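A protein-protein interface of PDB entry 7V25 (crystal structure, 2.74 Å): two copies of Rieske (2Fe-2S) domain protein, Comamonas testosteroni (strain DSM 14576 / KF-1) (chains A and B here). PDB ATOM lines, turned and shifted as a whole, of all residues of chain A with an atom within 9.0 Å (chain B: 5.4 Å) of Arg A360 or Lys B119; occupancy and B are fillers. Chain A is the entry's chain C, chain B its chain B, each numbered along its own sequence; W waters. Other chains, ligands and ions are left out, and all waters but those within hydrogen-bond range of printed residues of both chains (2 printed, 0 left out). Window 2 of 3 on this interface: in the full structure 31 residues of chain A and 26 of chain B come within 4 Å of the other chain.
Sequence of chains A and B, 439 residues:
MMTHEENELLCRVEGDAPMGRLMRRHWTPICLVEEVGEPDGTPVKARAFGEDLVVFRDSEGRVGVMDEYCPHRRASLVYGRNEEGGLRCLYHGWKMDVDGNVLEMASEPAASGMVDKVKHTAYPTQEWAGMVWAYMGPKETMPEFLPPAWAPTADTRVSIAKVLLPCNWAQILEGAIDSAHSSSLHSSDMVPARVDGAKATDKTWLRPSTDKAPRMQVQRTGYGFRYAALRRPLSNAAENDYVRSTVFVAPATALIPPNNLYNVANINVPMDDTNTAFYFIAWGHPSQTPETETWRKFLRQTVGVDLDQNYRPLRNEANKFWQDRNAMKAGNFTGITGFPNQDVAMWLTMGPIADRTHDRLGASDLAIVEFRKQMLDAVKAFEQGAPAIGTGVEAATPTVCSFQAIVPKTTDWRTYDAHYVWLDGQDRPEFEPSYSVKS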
ATOM      1  N   MET A   1      13.446 -27.095  20.607  1.00  0.00           N
ATOM      2  CA  MET A   1      13.585 -25.814  19.838  1.00  0.00           C
ATOM      3  C   MET A   1      12.781 -24.716  20.542  1.00  0.00           C
ATOM      4  O   MET A   1      11.775 -25.003  21.187  1.00  0.00           O
ATOM      5  CB  MET A   1      13.067 -26.012  18.412  1.00  0.00           C
ATOM      6  CG  MET A   1      13.375 -24.871  17.471  1.00  0.00           C
ATOM      7  SD  MET A   1      14.903 -25.149  16.543  1.00  0.00           S
ATOM      8  CE  MET A   1      16.133 -24.485  17.669  1.00  0.00           C
ATOM      9  N   ASP A 355      18.479 -14.327  17.471  1.00  0.00           N
ATOM     10  CA  ASP A 355      17.273 -15.087  17.174  1.00  0.00           C
ATOM     11  C   ASP A 355      17.598 -16.566  17.352  1.00  0.00           C
ATOM     12  O   ASP A 355      18.068 -17.214  16.422  1.00  0.00           O
ATOM     13  CB  ASP A 355      16.738 -14.768  15.765  1.00  0.00           C
ATOM     14  CG  ASP A 355      15.273 -15.099  15.481  1.00  0.00           C
ATOM     15  OD1 ASP A 355      14.591 -15.658  16.361  1.00  0.00           O
ATOM     16  OD2 ASP A 355      14.816 -14.788  14.363  1.00  0.00           O
ATOM     17  N   ARG A 356      17.347 -17.096  18.550  1.00  0.00           N
ATOM     18  CA  ARG A 356      17.667 -18.491  18.833  1.00  0.00           C
ATOM     19  C   ARG A 356      16.738 -19.438  18.058  1.00  0.00           C
ATOM     20  O   ARG A 356      17.053 -20.613  17.867  1.00  0.00           O
ATOM     21  CB  ARG A 356      17.693 -18.730  20.343  1.00  0.00           C
ATOM     22  CG  ARG A 356      18.753 -17.922  21.075  1.00  0.00           C
ATOM     23  CD  ARG A 356      18.525 -17.845  22.574  1.00  0.00           C
ATOM     24  NE  ARG A 356      19.643 -17.139  23.179  1.00  0.00           N
ATOM     25  CZ  ARG A 356      19.780 -15.821  23.208  1.00  0.00           C
ATOM     26  NH1 ARG A 356      18.855 -15.044  22.671  1.00  0.00           N
ATOM     27  NH2 ARG A 356      20.839 -15.279  23.782  1.00  0.00           N
ATOM     28  N   THR A 357      15.612 -18.894  17.584  1.00  0.00           N
ATOM     29  CA  THR A 357      14.645 -19.550  16.722  1.00  0.00           C
ATOM     30  C   THR A 357      15.325 -20.239  15.544  1.00  0.00           C
ATOM     31  O   THR A 357      14.912 -21.327  15.163  1.00  0.00           O
ATOM     32  CB  THR A 357      13.618 -18.524  16.240  1.00  0.00           C
ATOM     33  OG1 THR A 357      12.601 -18.488  17.246  1.00  0.00           O
ATOM     34  CG2 THR A 357      13.048 -18.815  14.867  1.00  0.00           C
ATOM     35  N   HIS A 358      16.358 -19.606  14.978  1.00  0.00           N
ATOM     36  CA  HIS A 358      17.043 -20.130  13.804  1.00  0.00           C
ATOM     37  C   HIS A 358      18.327 -20.874  14.182  1.00  0.00           C
ATOM     38  O   HIS A 358      19.147 -21.150  13.312  1.00  0.00           O
ATOM     39  CB  HIS A 358      17.308 -19.010  12.779  1.00  0.00           C
ATOM     40  CG  HIS A 358      16.087 -18.529  12.074  1.00  0.00           C
ATOM     41  ND1 HIS A 358      15.416 -17.376  12.457  1.00  0.00           N
ATOM     42  CD2 HIS A 358      15.403 -19.036  11.026  1.00  0.00           C
ATOM     43  CE1 HIS A 358      14.370 -17.193  11.674  1.00  0.00           C
ATOM     44  NE2 HIS A 358      14.343 -18.198  10.786  1.00  0.00           N
ATOM     45  N   ASP A 359      18.507 -21.216  15.467  1.00  0.00           N
ATOM     46  CA  ASP A 359      19.713 -21.926  15.874  1.00  0.00           C
ATOM     47  C   ASP A 359      19.569 -23.401  15.524  1.00  0.00           C
ATOM     48  O   ASP A 359      18.483 -23.947  15.681  1.00  0.00           O
ATOM     49  CB  ASP A 359      20.003 -21.753  17.369  1.00  0.00           C
ATOM     50  CG  ASP A 359      20.707 -20.453  17.723  1.00  0.00           C
ATOM     51  OD1 ASP A 359      21.083 -19.711  16.782  1.00  0.00           O
ATOM     52  OD2 ASP A 359      20.878 -20.188  18.937  1.00  0.00           O
ATOM     53  N   ARG A 360      20.654 -24.035  15.066  1.00  0.00           N
ATOM     54  CA  ARG A 360      20.669 -25.483  14.898  1.00  0.00           C
ATOM     55  C   ARG A 360      21.783 -26.084  15.743  1.00  0.00           C
ATOM     56  O   ARG A 360      22.880 -26.276  15.235  1.00  0.00           O
ATOM     57  CB  ARG A 360      20.970 -25.900  13.456  1.00  0.00           C
ATOM     58  CG  ARG A 360      20.065 -25.251  12.421  1.00  0.00           C
ATOM     59  CD  ARG A 360      20.448 -25.540  10.983  1.00  0.00           C
ATOM     60  NE  ARG A 360      19.670 -26.598  10.346  1.00  0.00           N
ATOM     61  CZ  ARG A 360      19.291 -26.575   9.069  1.00  0.00           C
ATOM     62  NH1 ARG A 360      19.604 -25.540   8.304  1.00  0.00           N
ATOM     63  NH2 ARG A 360      18.593 -27.576   8.561  1.00  0.00           N
ATOM     64  N   LEU A 361      21.478 -26.455  16.993  1.00  0.00           N
ATOM     65  CA  LEU A 361      22.493 -26.841  17.971  1.00  0.00           C
ATOM     66  C   LEU A 361      22.940 -28.304  17.866  1.00  0.00           C
ATOM     67  O   LEU A 361      22.381 -29.109  17.125  1.00  0.00           O
ATOM     68  CB  LEU A 361      21.951 -26.490  19.355  1.00  0.00           C
ATOM     69  CG  LEU A 361      21.647 -24.997  19.486  1.00  0.00           C
ATOM     70  CD1 LEU A 361      20.987 -24.649  20.813  1.00  0.00           C
ATOM     71  CD2 LEU A 361      22.913 -24.188  19.282  1.00  0.00           C
ATOM     72  N   GLY A 362      24.003 -28.631  18.599  1.00  0.00           N
ATOM     73  CA  GLY A 362      24.566 -29.974  18.588  1.00  0.00           C
ATOM     74  C   GLY A 362      25.174 -30.340  19.939  1.00  0.00           C
ATOM     75  O   GLY A 362      24.938 -29.647  20.928  1.00  0.00           O
ATOM     76  N   ALA A 363      25.957 -31.425  19.970  1.00  0.00           N
ATOM     77  CA  ALA A 363      26.574 -31.912  21.200  1.00  0.00           C
ATOM     78  C   ALA A 363      27.312 -30.786  21.916  1.00  0.00           C
ATOM     79  O   ALA A 363      27.106 -30.574  23.108  1.00  0.00           O
ATOM     80  CB  ALA A 363      27.508 -33.061  20.921  1.00  0.00           C
ATOM     81  N   SER A 364      28.142 -30.051  21.166  1.00  0.00           N
ATOM     82  CA  SER A 364      29.058 -29.091  21.753  1.00  0.00           C
ATOM     83  C   SER A 364      28.315 -27.962  22.466  1.00  0.00           C
ATOM     84  O   SER A 364      28.932 -27.142  23.145  1.00  0.00           O
ATOM     85  CB  SER A 364      30.017 -28.567  20.716  1.00  0.00           C
ATOM     86  OG  SER A 364      29.505 -27.400  20.078  1.00  0.00           O
ATOM     87  N   ASP A 365      26.990 -27.917  22.319  1.00  0.00           N
ATOM     88  CA  ASP A 365      26.260 -26.767  22.816  1.00  0.00           C
ATOM     89  C   ASP A 365      25.362 -27.190  23.971  1.00  0.00           C
ATOM     90  O   ASP A 365      24.341 -26.551  24.259  1.00  0.00           O
ATOM     91  CB  ASP A 365      25.485 -26.047  21.705  1.00  0.00           C
ATOM     92  CG  ASP A 365      26.332 -25.604  20.526  1.00  0.00           C
ATOM     93  OD1 ASP A 365      26.021 -26.062  19.406  1.00  0.00           O
ATOM     94  OD2 ASP A 365      27.296 -24.811  20.733  1.00  0.00           O
ATOM     95  N   VAL A 369      22.305 -25.064  25.829  1.00  0.00           N
ATOM     96  CA  VAL A 369      20.955 -25.597  25.953  1.00  0.00           C
ATOM     97  C   VAL A 369      20.520 -25.551  27.414  1.00  0.00           C
ATOM     98  O   VAL A 369      19.402 -25.149  27.722  1.00  0.00           O
ATOM     99  CB  VAL A 369      20.859 -27.047  25.455  1.00  0.00           C
ATOM    100  CG1 VAL A 369      19.423 -27.534  25.542  1.00  0.00           C
ATOM    101  CG2 VAL A 369      21.418 -27.218  24.050  1.00  0.00           C
ATOM    102  N   ARG A 372      19.540 -22.214  28.563  1.00  0.00           N
ATOM    103  CA  ARG A 372      18.267 -21.736  28.056  1.00  0.00           C
ATOM    104  C   ARG A 372      17.138 -22.390  28.847  1.00  0.00           C
ATOM    105  O   ARG A 372      16.158 -21.717  29.177  1.00  0.00           O
ATOM    106  CB  ARG A 372      18.144 -21.956  26.546  1.00  0.00           C
ATOM    107  CG  ARG A 372      19.214 -21.249  25.727  1.00  0.00           C
ATOM    108  CD  ARG A 372      19.530 -21.924  24.409  1.00  0.00           C
ATOM    109  NE  ARG A 372      20.365 -21.009  23.655  1.00  0.00           N
ATOM    110  CZ  ARG A 372      20.349 -20.870  22.332  1.00  0.00           C
ATOM    111  NH1 ARG A 372      19.515 -21.600  21.601  1.00  0.00           N
ATOM    112  NH2 ARG A 372      21.168 -19.997  21.757  1.00  0.00           N
ATOM    113  N   PRO B  71      24.931 -21.232   9.687  1.00  0.00           N
ATOM    114  CA  PRO B  71      23.810 -22.119  10.018  1.00  0.00           C
ATOM    115  C   PRO B  71      23.812 -22.618  11.466  1.00  0.00           C
ATOM    116  O   PRO B  71      22.796 -23.103  11.978  1.00  0.00           O
ATOM    117  CB  PRO B  71      23.963 -23.296   9.040  1.00  0.00           C
ATOM    118  CG  PRO B  71      25.421 -23.267   8.640  1.00  0.00           C
ATOM    119  CD  PRO B  71      25.813 -21.804   8.663  1.00  0.00           C
ATOM    120  N   HIS B  72      24.962 -22.485  12.134  1.00  0.00           N
ATOM    121  CA  HIS B  72      25.061 -22.880  13.524  1.00  0.00           C
ATOM    122  C   HIS B  72      24.336 -21.873  14.420  1.00  0.00           C
ATOM    123  O   HIS B  72      23.176 -22.105  14.797  1.00  0.00           O
ATOM    124  CB  HIS B  72      26.515 -23.147  13.913  1.00  0.00           C
ATOM    125  CG  HIS B  72      26.639 -23.652  15.310  1.00  0.00           C
ATOM    126  ND1 HIS B  72      27.728 -23.355  16.120  1.00  0.00           N
ATOM    127  CD2 HIS B  72      25.800 -24.396  16.062  1.00  0.00           C
ATOM    128  CE1 HIS B  72      27.569 -23.916  17.298  1.00  0.00           C
ATOM    129  NE2 HIS B  72      26.393 -24.557  17.282  1.00  0.00           N
ATOM    130  N   TRP B  94      32.410 -24.611  11.793  1.00  0.00           N
ATOM    131  CA  TRP B  94      31.626 -25.248  10.738  1.00  0.00           C
ATOM    132  C   TRP B  94      32.127 -24.716   9.405  1.00  0.00           C
ATOM    133  O   TRP B  94      32.314 -23.513   9.284  1.00  0.00           O
ATOM    134  CB  TRP B  94      30.124 -24.961  10.886  1.00  0.00           C
ATOM    135  CG  TRP B  94      29.391 -25.631  12.014  1.00  0.00           C
ATOM    136  CD1 TRP B  94      29.890 -26.060  13.213  1.00  0.00           C
ATOM    137  CD2 TRP B  94      27.975 -25.874  12.070  1.00  0.00           C
ATOM    138  NE1 TRP B  94      28.889 -26.561  14.005  1.00  0.00           N
ATOM    139  CE2 TRP B  94      27.704 -26.464  13.329  1.00  0.00           C
ATOM    140  CE3 TRP B  94      26.913 -25.672  11.173  1.00  0.00           C
ATOM    141  CZ2 TRP B  94      26.418 -26.860  13.700  1.00  0.00           C
ATOM    142  CZ3 TRP B  94      25.639 -26.059  11.543  1.00  0.00           C
ATOM    143  CH2 TRP B  94      25.403 -26.652  12.788  1.00  0.00           C
ATOM    144  N   GLY B 100      26.703 -24.749  -0.145  1.00  0.00           N
ATOM    145  CA  GLY B 100      26.001 -24.688   1.130  1.00  0.00           C
ATOM    146  C   GLY B 100      26.077 -26.003   1.910  1.00  0.00           C
ATOM    147  O   GLY B 100      25.377 -26.189   2.908  1.00  0.00           O
ATOM    148  N   ASN B 101      26.946 -26.899   1.433  1.00  0.00           N
ATOM    149  CA  ASN B 101      27.237 -28.158   2.088  1.00  0.00           C
ATOM    150  C   ASN B 101      28.179 -27.928   3.269  1.00  0.00           C
ATOM    151  O   ASN B 101      29.331 -27.518   3.089  1.00  0.00           O
ATOM    152  CB  ASN B 101      27.819 -29.157   1.088  1.00  0.00           C
ATOM    153  CG  ASN B 101      26.794 -29.591   0.063  1.00  0.00           C
ATOM    154  OD1 ASN B 101      25.717 -30.065   0.415  1.00  0.00           O
ATOM    155  ND2 ASN B 101      27.111 -29.427  -1.207  1.00  0.00           N
ATOM    156  N   VAL B 102      27.675 -28.196   4.480  1.00  0.00           N
ATOM    157  CA  VAL B 102      28.543 -28.226   5.643  1.00  0.00           C
ATOM    158  C   VAL B 102      29.520 -29.381   5.450  1.00  0.00           C
ATOM    159  O   VAL B 102      29.133 -30.535   5.618  1.00  0.00           O
ATOM    160  CB  VAL B 102      27.742 -28.364   6.953  1.00  0.00           C
ATOM    161  CG1 VAL B 102      28.643 -28.307   8.174  1.00  0.00           C
ATOM    162  CG2 VAL B 102      26.631 -27.329   7.073  1.00  0.00           C
ATOM    163  N   MET B 114      25.083 -35.704  11.819  1.00  0.00           N
ATOM    164  CA  MET B 114      24.577 -34.344  11.722  1.00  0.00           C
ATOM    165  C   MET B 114      25.397 -33.548  10.701  1.00  0.00           C
ATOM    166  O   MET B 114      25.013 -32.440  10.333  1.00  0.00           O
ATOM    167  CB  MET B 114      24.631 -33.651  13.093  1.00  0.00           C
ATOM    168  CG  MET B 114      23.576 -32.562  13.302  1.00  0.00           C
ATOM    169  SD  MET B 114      24.109 -31.169  14.355  1.00  0.00           S
ATOM    170  CE  MET B 114      22.742 -30.033  14.114  1.00  0.00           C
ATOM    171  N   ASP B 116      26.167 -33.922   7.422  1.00  0.00           N
ATOM    172  CA  ASP B 116      25.700 -33.670   6.064  1.00  0.00           C
ATOM    173  C   ASP B 116      24.171 -33.691   5.975  1.00  0.00           C
ATOM    174  O   ASP B 116      23.623 -33.780   4.876  1.00  0.00           O
ATOM    175  CB  ASP B 116      26.440 -34.522   5.018  1.00  0.00           C
ATOM    176  CG  ASP B 116      26.768 -35.951   5.437  1.00  0.00           C
ATOM    177  OD1 ASP B 116      27.826 -36.461   5.006  1.00  0.00           O
ATOM    178  OD2 ASP B 116      25.964 -36.552   6.175  1.00  0.00           O
ATOM    179  N   LYS B 117      23.490 -33.587   7.127  1.00  0.00           N
ATOM    180  CA  LYS B 117      22.044 -33.393   7.158  1.00  0.00           C
ATOM    181  C   LYS B 117      21.726 -31.893   7.154  1.00  0.00           C
ATOM    182  O   LYS B 117      20.768 -31.470   6.510  1.00  0.00           O
ATOM    183  CB  LYS B 117      21.365 -34.188   8.286  1.00  0.00           C
ATOM    184  CG  LYS B 117      21.664 -33.730   9.711  1.00  0.00           C
ATOM    185  CD  LYS B 117      20.707 -34.227  10.789  1.00  0.00           C
ATOM    186  CE  LYS B 117      21.015 -35.611  11.325  1.00  0.00           C
ATOM    187  NZ  LYS B 117      20.897 -35.678  12.802  1.00  0.00           N
ATOM    188  N   VAL B 118      22.546 -31.102   7.868  1.00  0.00           N
ATOM    189  CA  VAL B 118      22.459 -29.646   7.874  1.00  0.00           C
ATOM    190  C   VAL B 118      22.925 -29.123   6.514  1.00  0.00           C
ATOM    191  O   VAL B 118      24.010 -29.475   6.043  1.00  0.00           O
ATOM    192  CB  VAL B 118      23.264 -29.008   9.031  1.00  0.00           C
ATOM    193  CG1 VAL B 118      23.452 -27.515   8.840  1.00  0.00           C
ATOM    194  CG2 VAL B 118      22.649 -29.261  10.397  1.00  0.00           C
ATOM    195  N   LYS B 119      22.084 -28.274   5.906  1.00  0.00           N
ATOM    196  CA  LYS B 119      22.429 -27.548   4.691  1.00  0.00           C
ATOM    197  C   LYS B 119      22.166 -26.049   4.873  1.00  0.00           C
ATOM    198  O   LYS B 119      21.211 -25.665   5.539  1.00  0.00           O
ATOM    199  CB  LYS B 119      21.661 -28.139   3.505  1.00  0.00           C
ATOM    200  CG  LYS B 119      21.858 -29.635   3.281  1.00  0.00           C
ATOM    201  CD  LYS B 119      23.039 -29.968   2.395  1.00  0.00           C
ATOM    202  CE  LYS B 119      23.032 -31.406   1.916  1.00  0.00           C
ATOM    203  NZ  LYS B 119      23.557 -32.339   2.942  1.00  0.00           N
ATOM    204  N   HIS B 120      23.026 -25.207   4.281  1.00  0.00           N
ATOM    205  CA  HIS B 120      22.951 -23.759   4.424  1.00  0.00           C
ATOM    206  C   HIS B 120      22.434 -23.130   3.133  1.00  0.00           C
ATOM    207  O   HIS B 120      22.724 -23.617   2.040  1.00  0.00           O
ATOM    208  CB  HIS B 120      24.344 -23.207   4.715  1.00  0.00           C
ATOM    209  CG  HIS B 120      24.376 -21.740   5.000  1.00  0.00           C
ATOM    210  ND1 HIS B 120      23.573 -21.144   5.972  1.00  0.00           N
ATOM    211  CD2 HIS B 120      25.136 -20.750   4.483  1.00  0.00           C
ATOM    212  CE1 HIS B 120      23.827 -19.848   6.016  1.00  0.00           C
ATOM    213  NE2 HIS B 120      24.786 -19.582   5.113  1.00  0.00           N
ATOM    214  N   THR B 121      21.696 -22.028   3.262  1.00  0.00           N
ATOM    215  CA  THR B 121      21.104 -21.368   2.112  1.00  0.00           C
ATOM    216  C   THR B 121      22.196 -20.851   1.182  1.00  0.00           C
ATOM    217  O   THR B 121      22.930 -19.934   1.540  1.00  0.00           O
ATOM    218  CB  THR B 121      20.204 -20.203   2.557  1.00  0.00           C
ATOM    219  OG1 THR B 121      19.464 -20.634   3.703  1.00  0.00           O
ATOM    220  CG2 THR B 121      19.293 -19.667   1.467  1.00  0.00           C
HETATM  221  O   HOH W   1      20.265 -21.562  10.847  1.00  0.00           O
HETATM  222  O   HOH W   2      29.005 -27.030  17.328  1.00  0.00           O
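Of the printed residues of chain B, Arg A360 touches Pro B71, His B72, Trp B94, Met B114, Val B118 and Lys B119.
Of the printed residues of chain A, Lys B119 touches Arg A360.
Of the printed residues of chain A, Pro B71 touches Arg A360 (3.5 Å).
Of the printed residues of chain B, Asp A365 touches His B72.
Of the printed residues of chain A, Val B118 touches Arg A360 (3.996 Å).
Of the printed residues of chain A, His B72 touches Asp A359 (3.6 Å), Arg A360 (3.2 Å) and Asp A365 (2.6 Å).
The nearest printed residue of chain A that does not touch Lys B119 is His A358 (9.2 Å).
The nearest printed residue of chain A that does not touch His B72 is Leu A361 (4.03 Å).
No position is printed for both chains.
Of the 9 pairs that touch across the chains among the printed residues, none has its exchanged pair printed and touching as well.
Water W1 lies within hydrogen-bond range of O of His A358 (2.7 Å) and O of Pro B71 (3.2 Å).
Water W2 bridges the side-chain hydroxyl of Ser A364 (2.8 Å) and the indole nitrogen of Trp B94 (3.4 Å).
O of His B72 is in hydrogen-bond range of N of Arg A360, 3.2 Å away.
The guanidinium group of Arg A360 sits at hydrogen-bond distance from the backbone carbonyl oxygen of Lys B119 (3.2 Å).
OD1 of Asp A365 lies within hydrogen-bond range of NE2 of His B72, at 2.6 Å.
Hydrophobic or aromatic side chains of chain B that line the printed part of chain A: His B72, Trp B94, Met B114 and Val B118.
Of the 14 printed residues of chain A, 4 touch a printed residue of chain B.
Among the printed residues, no Asp or Glu carboxylate lies within 4 Å of a Lys or Arg side-chain nitrogen of the other chain.
N of Gly A362 lies within hydrogen-bond range of OD1 of Asp A365.
The side-chain carboxylate (OD2) of Asp A359 lies within salt-bridge range of the guanidinium group (NH2) of Arg A372 (2.8 Å).
The backbone carbonyl oxygen of Asp B116 sits at hydrogen-bond distance from the side-chain amino group of Lys B119 (2.4 Å).
The side-chain hydroxyl of Ser A364 lies within hydrogen-bond range of the side-chain carboxylate of Asp A365.
Among the printed residues, merely in contact across the chains: Asp A359 with His B72, Arg A360 with Pro B71, Arg A360 with Trp B94, Arg A360 with Met B114, Arg A360 with Val B118 and Leu A361 with Met B114.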
